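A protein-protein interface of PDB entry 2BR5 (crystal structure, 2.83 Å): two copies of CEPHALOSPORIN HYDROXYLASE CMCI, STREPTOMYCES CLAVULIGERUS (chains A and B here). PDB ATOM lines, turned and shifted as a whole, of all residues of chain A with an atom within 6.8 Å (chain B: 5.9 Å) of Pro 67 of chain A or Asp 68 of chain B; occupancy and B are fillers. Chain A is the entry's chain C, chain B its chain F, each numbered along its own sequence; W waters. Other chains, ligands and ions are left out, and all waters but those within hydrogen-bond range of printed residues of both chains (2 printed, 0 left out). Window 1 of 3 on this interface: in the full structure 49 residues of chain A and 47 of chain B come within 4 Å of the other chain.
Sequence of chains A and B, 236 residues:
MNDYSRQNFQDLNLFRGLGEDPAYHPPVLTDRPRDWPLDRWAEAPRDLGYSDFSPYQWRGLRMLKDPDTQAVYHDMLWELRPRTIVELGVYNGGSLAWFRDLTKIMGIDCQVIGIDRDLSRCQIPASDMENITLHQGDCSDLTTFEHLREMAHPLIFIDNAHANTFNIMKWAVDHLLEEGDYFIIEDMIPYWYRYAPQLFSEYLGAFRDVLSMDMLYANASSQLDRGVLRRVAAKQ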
ATOM      1  N   TYR A  56      -1.232   5.741   9.480  1.00  0.00           N
ATOM      2  CA  TYR A  56      -1.431   5.266  10.837  1.00  0.00           C
ATOM      3  C   TYR A  56      -0.210   4.546  11.425  1.00  0.00           C
ATOM      4  O   TYR A  56       0.622   4.008  10.706  1.00  0.00           O
ATOM      5  CB  TYR A  56      -2.685   4.416  10.861  1.00  0.00           C
ATOM      6  CG  TYR A  56      -3.892   5.188  10.398  1.00  0.00           C
ATOM      7  CD1 TYR A  56      -4.531   4.885   9.184  1.00  0.00           C
ATOM      8  CD2 TYR A  56      -4.391   6.246  11.164  1.00  0.00           C
ATOM      9  CE1 TYR A  56      -5.655   5.606   8.760  1.00  0.00           C
ATOM     10  CE2 TYR A  56      -5.507   6.977  10.758  1.00  0.00           C
ATOM     11  CZ  TYR A  56      -6.141   6.657   9.558  1.00  0.00           C
ATOM     12  OH  TYR A  56      -7.242   7.396   9.166  1.00  0.00           O
ATOM     13  N   MET A  63       1.084   1.177  10.687  1.00  0.00           N
ATOM     14  CA  MET A  63      -0.137   0.401  10.861  1.00  0.00           C
ATOM     15  C   MET A  63      -0.918   0.537   9.584  1.00  0.00           C
ATOM     16  O   MET A  63      -1.345   1.640   9.239  1.00  0.00           O
ATOM     17  CB  MET A  63      -0.989   0.959  11.989  1.00  0.00           C
ATOM     18  CG  MET A  63      -0.803   0.253  13.303  1.00  0.00           C
ATOM     19  SD  MET A  63      -1.420  -1.434  13.343  1.00  0.00           S
ATOM     20  CE  MET A  63      -3.089  -1.194  12.881  1.00  0.00           C
ATOM     21  N   LYS A  65      -3.792  -1.262   9.177  1.00  0.00           N
ATOM     22  CA  LYS A  65      -5.194  -1.373   9.550  1.00  0.00           C
ATOM     23  C   LYS A  65      -5.647  -0.023  10.053  1.00  0.00           C
ATOM     24  O   LYS A  65      -5.065   0.517  10.969  1.00  0.00           O
ATOM     25  CB  LYS A  65      -5.408  -2.426  10.638  1.00  0.00           C
ATOM     26  CG  LYS A  65      -4.752  -3.744  10.373  1.00  0.00           C
ATOM     27  CD  LYS A  65      -5.531  -4.842  10.984  1.00  0.00           C
ATOM     28  CE  LYS A  65      -4.832  -6.172  10.822  1.00  0.00           C
ATOM     29  NZ  LYS A  65      -4.453  -6.483   9.393  1.00  0.00           N
ATOM     30  N   ASP A  66      -6.679   0.541   9.461  1.00  0.00           N
ATOM     31  CA  ASP A  66      -7.071   1.876   9.837  1.00  0.00           C
ATOM     32  C   ASP A  66      -7.826   1.819  11.163  1.00  0.00           C
ATOM     33  O   ASP A  66      -8.080   0.733  11.661  1.00  0.00           O
ATOM     34  CB  ASP A  66      -7.831   2.538   8.699  1.00  0.00           C
ATOM     35  CG  ASP A  66      -9.104   1.844   8.369  1.00  0.00           C
ATOM     36  OD1 ASP A  66      -9.807   1.414   9.316  1.00  0.00           O
ATOM     37  OD2 ASP A  66      -9.483   1.702   7.187  1.00  0.00           O
ATOM     38  N   PRO A  67      -8.106   2.967  11.776  1.00  0.00           N
ATOM     39  CA  PRO A  67      -8.713   3.010  13.116  1.00  0.00           C
ATOM     40  C   PRO A  67     -10.059   2.301  13.252  1.00  0.00           C
ATOM     41  O   PRO A  67     -10.374   1.740  14.299  1.00  0.00           O
ATOM     42  CB  PRO A  67      -8.906   4.502  13.350  1.00  0.00           C
ATOM     43  CG  PRO A  67      -7.886   5.138  12.506  1.00  0.00           C
ATOM     44  CD  PRO A  67      -7.824   4.323  11.269  1.00  0.00           C
ATOM     45  N   ASP A  68     -10.865   2.336  12.204  1.00  0.00           N
ATOM     46  CA  ASP A  68     -12.142   1.652  12.261  1.00  0.00           C
ATOM     47  C   ASP A  68     -11.912   0.140  12.397  1.00  0.00           C
ATOM     48  O   ASP A  68     -12.510  -0.519  13.264  1.00  0.00           O
ATOM     49  CB  ASP A  68     -12.983   1.995  11.038  1.00  0.00           C
ATOM     50  CG  ASP A  68     -13.522   3.409  11.098  1.00  0.00           C
ATOM     51  OD1 ASP A  68     -12.978   4.297  10.396  1.00  0.00           O
ATOM     52  OD2 ASP A  68     -14.472   3.737  11.844  1.00  0.00           O
ATOM     53  N   THR A  69     -11.031  -0.400  11.561  1.00  0.00           N
ATOM     54  CA  THR A  69     -10.693  -1.810  11.646  1.00  0.00           C
ATOM     55  C   THR A  69     -10.190  -2.127  13.054  1.00  0.00           C
ATOM     56  O   THR A  69     -10.530  -3.163  13.608  1.00  0.00           O
ATOM     57  CB  THR A  69      -9.629  -2.187  10.570  1.00  0.00           C
ATOM     58  OG1 THR A  69     -10.216  -2.162   9.264  1.00  0.00           O
ATOM     59  CG2 THR A  69      -9.172  -3.634  10.714  1.00  0.00           C
ATOM     60  N   GLN A  70      -9.400  -1.222  13.631  1.00  0.00           N
ATOM     61  CA  GLN A  70      -8.773  -1.478  14.921  1.00  0.00           C
ATOM     62  C   GLN A  70      -9.820  -1.566  16.008  1.00  0.00           C
ATOM     63  O   GLN A  70      -9.727  -2.394  16.890  1.00  0.00           O
ATOM     64  CB  GLN A  70      -7.757  -0.385  15.272  1.00  0.00           C
ATOM     65  CG  GLN A  70      -6.491  -0.323  14.381  1.00  0.00           C
ATOM     66  CD  GLN A  70      -5.648   0.912  14.682  1.00  0.00           C
ATOM     67  OE1 GLN A  70      -5.520   1.311  15.864  1.00  0.00           O
ATOM     68  NE2 GLN A  70      -5.092   1.532  13.638  1.00  0.00           N
ATOM     69  N   ALA A  71     -10.813  -0.694  15.937  1.00  0.00           N
ATOM     70  CA  ALA A  71     -11.943  -0.731  16.844  1.00  0.00           C
ATOM     71  C   ALA A  71     -12.633  -2.093  16.772  1.00  0.00           C
ATOM     72  O   ALA A  71     -12.953  -2.685  17.797  1.00  0.00           O
ATOM     73  CB  ALA A  71     -12.914   0.359  16.495  1.00  0.00           C
ATOM     74  N   VAL A  72     -12.855  -2.604  15.569  1.00  0.00           N
ATOM     75  CA  VAL A  72     -13.478  -3.911  15.425  1.00  0.00           C
ATOM     76  C   VAL A  72     -12.634  -4.984  16.134  1.00  0.00           C
ATOM     77  O   VAL A  72     -13.157  -5.727  16.953  1.00  0.00           O
ATOM     78  CB  VAL A  72     -13.740  -4.272  13.935  1.00  0.00           C
ATOM     79  CG1 VAL A  72     -14.268  -5.689  13.795  1.00  0.00           C
ATOM     80  CG2 VAL A  72     -14.728  -3.280  13.300  1.00  0.00           C
ATOM     81  N   GLN A 223     -12.293  -2.190   5.628  1.00  0.00           N
ATOM     82  CA  GLN A 223     -11.296  -3.231   5.294  1.00  0.00           C
ATOM     83  C   GLN A 223     -11.768  -4.653   5.599  1.00  0.00           C
ATOM     84  O   GLN A 223     -11.391  -5.580   4.885  1.00  0.00           O
ATOM     85  CB  GLN A 223      -9.946  -2.996   6.002  1.00  0.00           C
ATOM     86  CG  GLN A 223      -9.272  -1.665   5.654  1.00  0.00           C
ATOM     87  CD  GLN A 223      -8.129  -1.291   6.586  1.00  0.00           C
ATOM     88  OE1 GLN A 223      -8.230  -1.418   7.797  1.00  0.00           O
ATOM     89  NE2 GLN A 223      -7.041  -0.839   6.014  1.00  0.00           N
ATOM     90  N   ASP B  66     -14.162   8.382  19.415  1.00  0.00           N
ATOM     91  CA  ASP B  66     -14.269   7.534  18.235  1.00  0.00           C
ATOM     92  C   ASP B  66     -12.858   7.215  17.694  1.00  0.00           C
ATOM     93  O   ASP B  66     -11.886   7.836  18.107  1.00  0.00           O
ATOM     94  CB  ASP B  66     -15.267   8.116  17.206  1.00  0.00           C
ATOM     95  CG  ASP B  66     -14.832   9.430  16.614  1.00  0.00           C
ATOM     96  OD1 ASP B  66     -13.613   9.660  16.412  1.00  0.00           O
ATOM     97  OD2 ASP B  66     -15.678  10.292  16.275  1.00  0.00           O
ATOM     98  N   PRO B  67     -12.733   6.200  16.838  1.00  0.00           N
ATOM     99  CA  PRO B  67     -11.409   5.658  16.490  1.00  0.00           C
ATOM    100  C   PRO B  67     -10.441   6.685  15.932  1.00  0.00           C
ATOM    101  O   PRO B  67      -9.227   6.513  16.127  1.00  0.00           O
ATOM    102  CB  PRO B  67     -11.734   4.574  15.453  1.00  0.00           C
ATOM    103  CG  PRO B  67     -13.132   4.154  15.796  1.00  0.00           C
ATOM    104  CD  PRO B  67     -13.815   5.455  16.164  1.00  0.00           C
ATOM    105  N   ASP B  68     -10.950   7.736  15.290  1.00  0.00           N
ATOM    106  CA  ASP B  68     -10.079   8.775  14.737  1.00  0.00           C
ATOM    107  C   ASP B  68      -9.480   9.652  15.816  1.00  0.00           C
ATOM    108  O   ASP B  68      -8.353  10.095  15.710  1.00  0.00           O
ATOM    109  CB  ASP B  68     -10.838   9.610  13.719  1.00  0.00           C
ATOM    110  CG  ASP B  68     -11.402   8.755  12.607  1.00  0.00           C
ATOM    111  OD1 ASP B  68     -12.501   9.063  12.111  1.00  0.00           O
ATOM    112  OD2 ASP B  68     -10.829   7.715  12.192  1.00  0.00           O
ATOM    113  N   THR B  69     -10.242   9.895  16.861  1.00  0.00           N
ATOM    114  CA  THR B  69      -9.727  10.585  18.023  1.00  0.00           C
ATOM    115  C   THR B  69      -8.673   9.755  18.720  1.00  0.00           C
ATOM    116  O   THR B  69      -7.655  10.271  19.147  1.00  0.00           O
ATOM    117  CB  THR B  69     -10.882  10.910  18.950  1.00  0.00           C
ATOM    118  OG1 THR B  69     -11.779  11.800  18.263  1.00  0.00           O
ATOM    119  CG2 THR B  69     -10.424  11.705  20.157  1.00  0.00           C
ATOM    120  N   GLN B  70      -8.920   8.458  18.811  1.00  0.00           N
ATOM    121  CA  GLN B  70      -7.964   7.513  19.394  1.00  0.00           C
ATOM    122  C   GLN B  70      -6.618   7.534  18.666  1.00  0.00           C
ATOM    123  O   GLN B  70      -5.554   7.409  19.282  1.00  0.00           O
ATOM    124  CB  GLN B  70      -8.543   6.100  19.353  1.00  0.00           C
ATOM    125  CG  GLN B  70      -9.580   5.846  20.437  1.00  0.00           C
ATOM    126  CD  GLN B  70     -10.164   4.445  20.390  1.00  0.00           C
ATOM    127  OE1 GLN B  70      -9.500   3.493  19.951  1.00  0.00           O
ATOM    128  NE2 GLN B  70     -11.410   4.316  20.825  1.00  0.00           N
ATOM    129  N   ALA B  71      -6.669   7.690  17.350  1.00  0.00           N
ATOM    130  CA  ALA B  71      -5.467   7.631  16.557  1.00  0.00           C
ATOM    131  C   ALA B  71      -4.675   8.910  16.759  1.00  0.00           C
ATOM    132  O   ALA B  71      -3.464   8.855  16.962  1.00  0.00           O
ATOM    133  CB  ALA B  71      -5.814   7.434  15.107  1.00  0.00           C
ATOM    134  N   VAL B  72      -5.349  10.059  16.715  1.00  0.00           N
ATOM    135  CA  VAL B  72      -4.694  11.336  16.982  1.00  0.00           C
ATOM    136  C   VAL B  72      -4.045  11.339  18.362  1.00  0.00           C
ATOM    137  O   VAL B  72      -2.891  11.715  18.498  1.00  0.00           O
ATOM    138  CB  VAL B  72      -5.668  12.517  16.891  1.00  0.00           C
ATOM    139  CG1 VAL B  72      -5.006  13.789  17.375  1.00  0.00           C
ATOM    140  CG2 VAL B  72      -6.152  12.704  15.466  1.00  0.00           C
ATOM    141  N   TYR B  73      -4.791  10.910  19.379  1.00  0.00           N
ATOM    142  CA  TYR B  73      -4.261  10.809  20.743  1.00  0.00           C
ATOM    143  C   TYR B  73      -3.103   9.845  20.846  1.00  0.00           C
ATOM    144  O   TYR B  73      -2.162  10.094  21.571  1.00  0.00           O
ATOM    145  CB  TYR B  73      -5.344  10.405  21.744  1.00  0.00           C
ATOM    146  CG  TYR B  73      -6.142  11.571  22.282  1.00  0.00           C
ATOM    147  CD1 TYR B  73      -7.527  11.558  22.223  1.00  0.00           C
ATOM    148  CD2 TYR B  73      -5.516  12.690  22.837  1.00  0.00           C
ATOM    149  CE1 TYR B  73      -8.275  12.616  22.698  1.00  0.00           C
ATOM    150  CE2 TYR B  73      -6.267  13.771  23.318  1.00  0.00           C
ATOM    151  CZ  TYR B  73      -7.647  13.721  23.245  1.00  0.00           C
ATOM    152  OH  TYR B  73      -8.419  14.751  23.715  1.00  0.00           O
ATOM    153  N   ALA B 220      -7.563  16.179  11.957  1.00  0.00           N
ATOM    154  CA  ALA B 220      -7.486  14.729  11.778  1.00  0.00           C
ATOM    155  C   ALA B 220      -8.611  13.974  12.475  1.00  0.00           C
ATOM    156  O   ALA B 220      -8.591  12.745  12.529  1.00  0.00           O
ATOM    157  CB  ALA B 220      -6.130  14.219  12.259  1.00  0.00           C
ATOM    158  N   SER B 221      -9.583  14.702  13.009  1.00  0.00           N
ATOM    159  CA  SER B 221     -10.693  14.091  13.730  1.00  0.00           C
ATOM    160  C   SER B 221     -11.877  15.031  13.831  1.00  0.00           C
ATOM    161  O   SER B 221     -11.712  16.220  14.076  1.00  0.00           O
ATOM    162  CB  SER B 221     -10.274  13.733  15.142  1.00  0.00           C
ATOM    163  OG  SER B 221     -11.409  13.669  15.988  1.00  0.00           O
ATOM    164  N   SER B 222     -13.078  14.495  13.674  1.00  0.00           N
ATOM    165  CA  SER B 222     -14.268  15.314  13.808  1.00  0.00           C
ATOM    166  C   SER B 222     -14.399  15.861  15.250  1.00  0.00           C
ATOM    167  O   SER B 222     -14.752  17.020  15.423  1.00  0.00           O
ATOM    168  CB  SER B 222     -15.522  14.559  13.315  1.00  0.00           C
ATOM    169  OG  SER B 222     -16.254  13.969  14.368  1.00  0.00           O
ATOM    170  N   LEU B 224     -11.928  16.392  17.637  1.00  0.00           N
ATOM    171  CA  LEU B 224     -10.901  17.369  18.044  1.00  0.00           C
ATOM    172  C   LEU B 224     -10.745  18.469  17.016  1.00  0.00           C
ATOM    173  O   LEU B 224      -9.869  19.310  17.136  1.00  0.00           O
ATOM    174  CB  LEU B 224      -9.543  16.705  18.260  1.00  0.00           C
ATOM    175  CG  LEU B 224      -9.516  15.374  18.989  1.00  0.00           C
ATOM    176  CD1 LEU B 224      -8.098  14.871  19.021  1.00  0.00           C
ATOM    177  CD2 LEU B 224     -10.106  15.517  20.391  1.00  0.00           C
HETATM  178  O   HOH W   1      -9.299   2.869  16.704  1.00  0.00           O
HETATM  179  O   HOH W   2      -8.407   8.848  11.106  1.00  0.00           O
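Among the printed residues, merely in contact across the chains: Pro 67 of chain A with Pro 67 of chain B, Pro 67 of chain A with Asp 68 of chain B and Ala 71 of chain A with Pro 67 of chain B.
Water W2 bridges the side-chain hydroxyl (OH) of Tyr 56 of chain A (2.7 Å) and the side-chain carboxylate (OD2) of Asp 68 of chain B (2.9 Å).
Water W1 bridges O of Pro 67 of chain A and OE1 of Gln 70 of chain B.
The side-chain carboxylate of Asp 66 of chain B sits close to the backbone NH of Asp 68 of chain B.
Of the 11 printed residues of chain A, 2 touch a printed residue of chain B.
Printed residues of chain A that touch a printed residue of chain B: Pro 67 and Ala 71.
Hydrophobic or aromatic side chains of chain A that line the printed part of chain B: Pro 67 and Ala 71.
Hydrophobic or aromatic side chains of chain B within 4 Å of the printed part of chain A: Pro 67.
Among the printed residues, no Asp or Glu carboxylate lies within 4 Å of a Lys or Arg side-chain nitrogen of the other chain.
Of the printed residues of chain B, Pro 67 of chain A touches Pro 67 (3.3 Å) and Asp 68 (3.9 Å).
Printed residues of chain B within 4 Å of Ala 71 of chain A: Pro 67.
Gln 223 of chain A touches none of the printed residues of chain B.
Printed residues of chain A within 4 Å of Pro 67 of chain B: Pro 67 (3.3 Å) and Ala 71 (3.9 Å).
Printed residues of chain A within 4 Å of Asp 68 of chain B: Pro 67 (3.9 Å).
Tyr 73 of chain B touches none of the printed residues of chain A.
The nearest residue of chain B that does not touch Pro 67 of chain A is Ala 71 of chain B (4.04 Å).
The nearest printed residue of chain B that does not touch Ala 71 of chain A is Gln 70 of chain B (5.8 Å).
Pro 67 of chain B touches its own counterpart, Pro 67 of chain A.
Pro 67 of chain A touches Asp 68 of chain B, but with the chains exchanged Asp 68 of chain A does not touch Pro 67 of chain B (4.04 Å).
Ala 71 of chain A touches Pro 67 of chain B, but with the chains exchanged Pro 67 of chain A does not touch Ala 71 of chain B (4.04 Å).
Of the 3 pairs that touch across the chains among the printed residues, 1 has its exchanged pair printed and touching as well.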
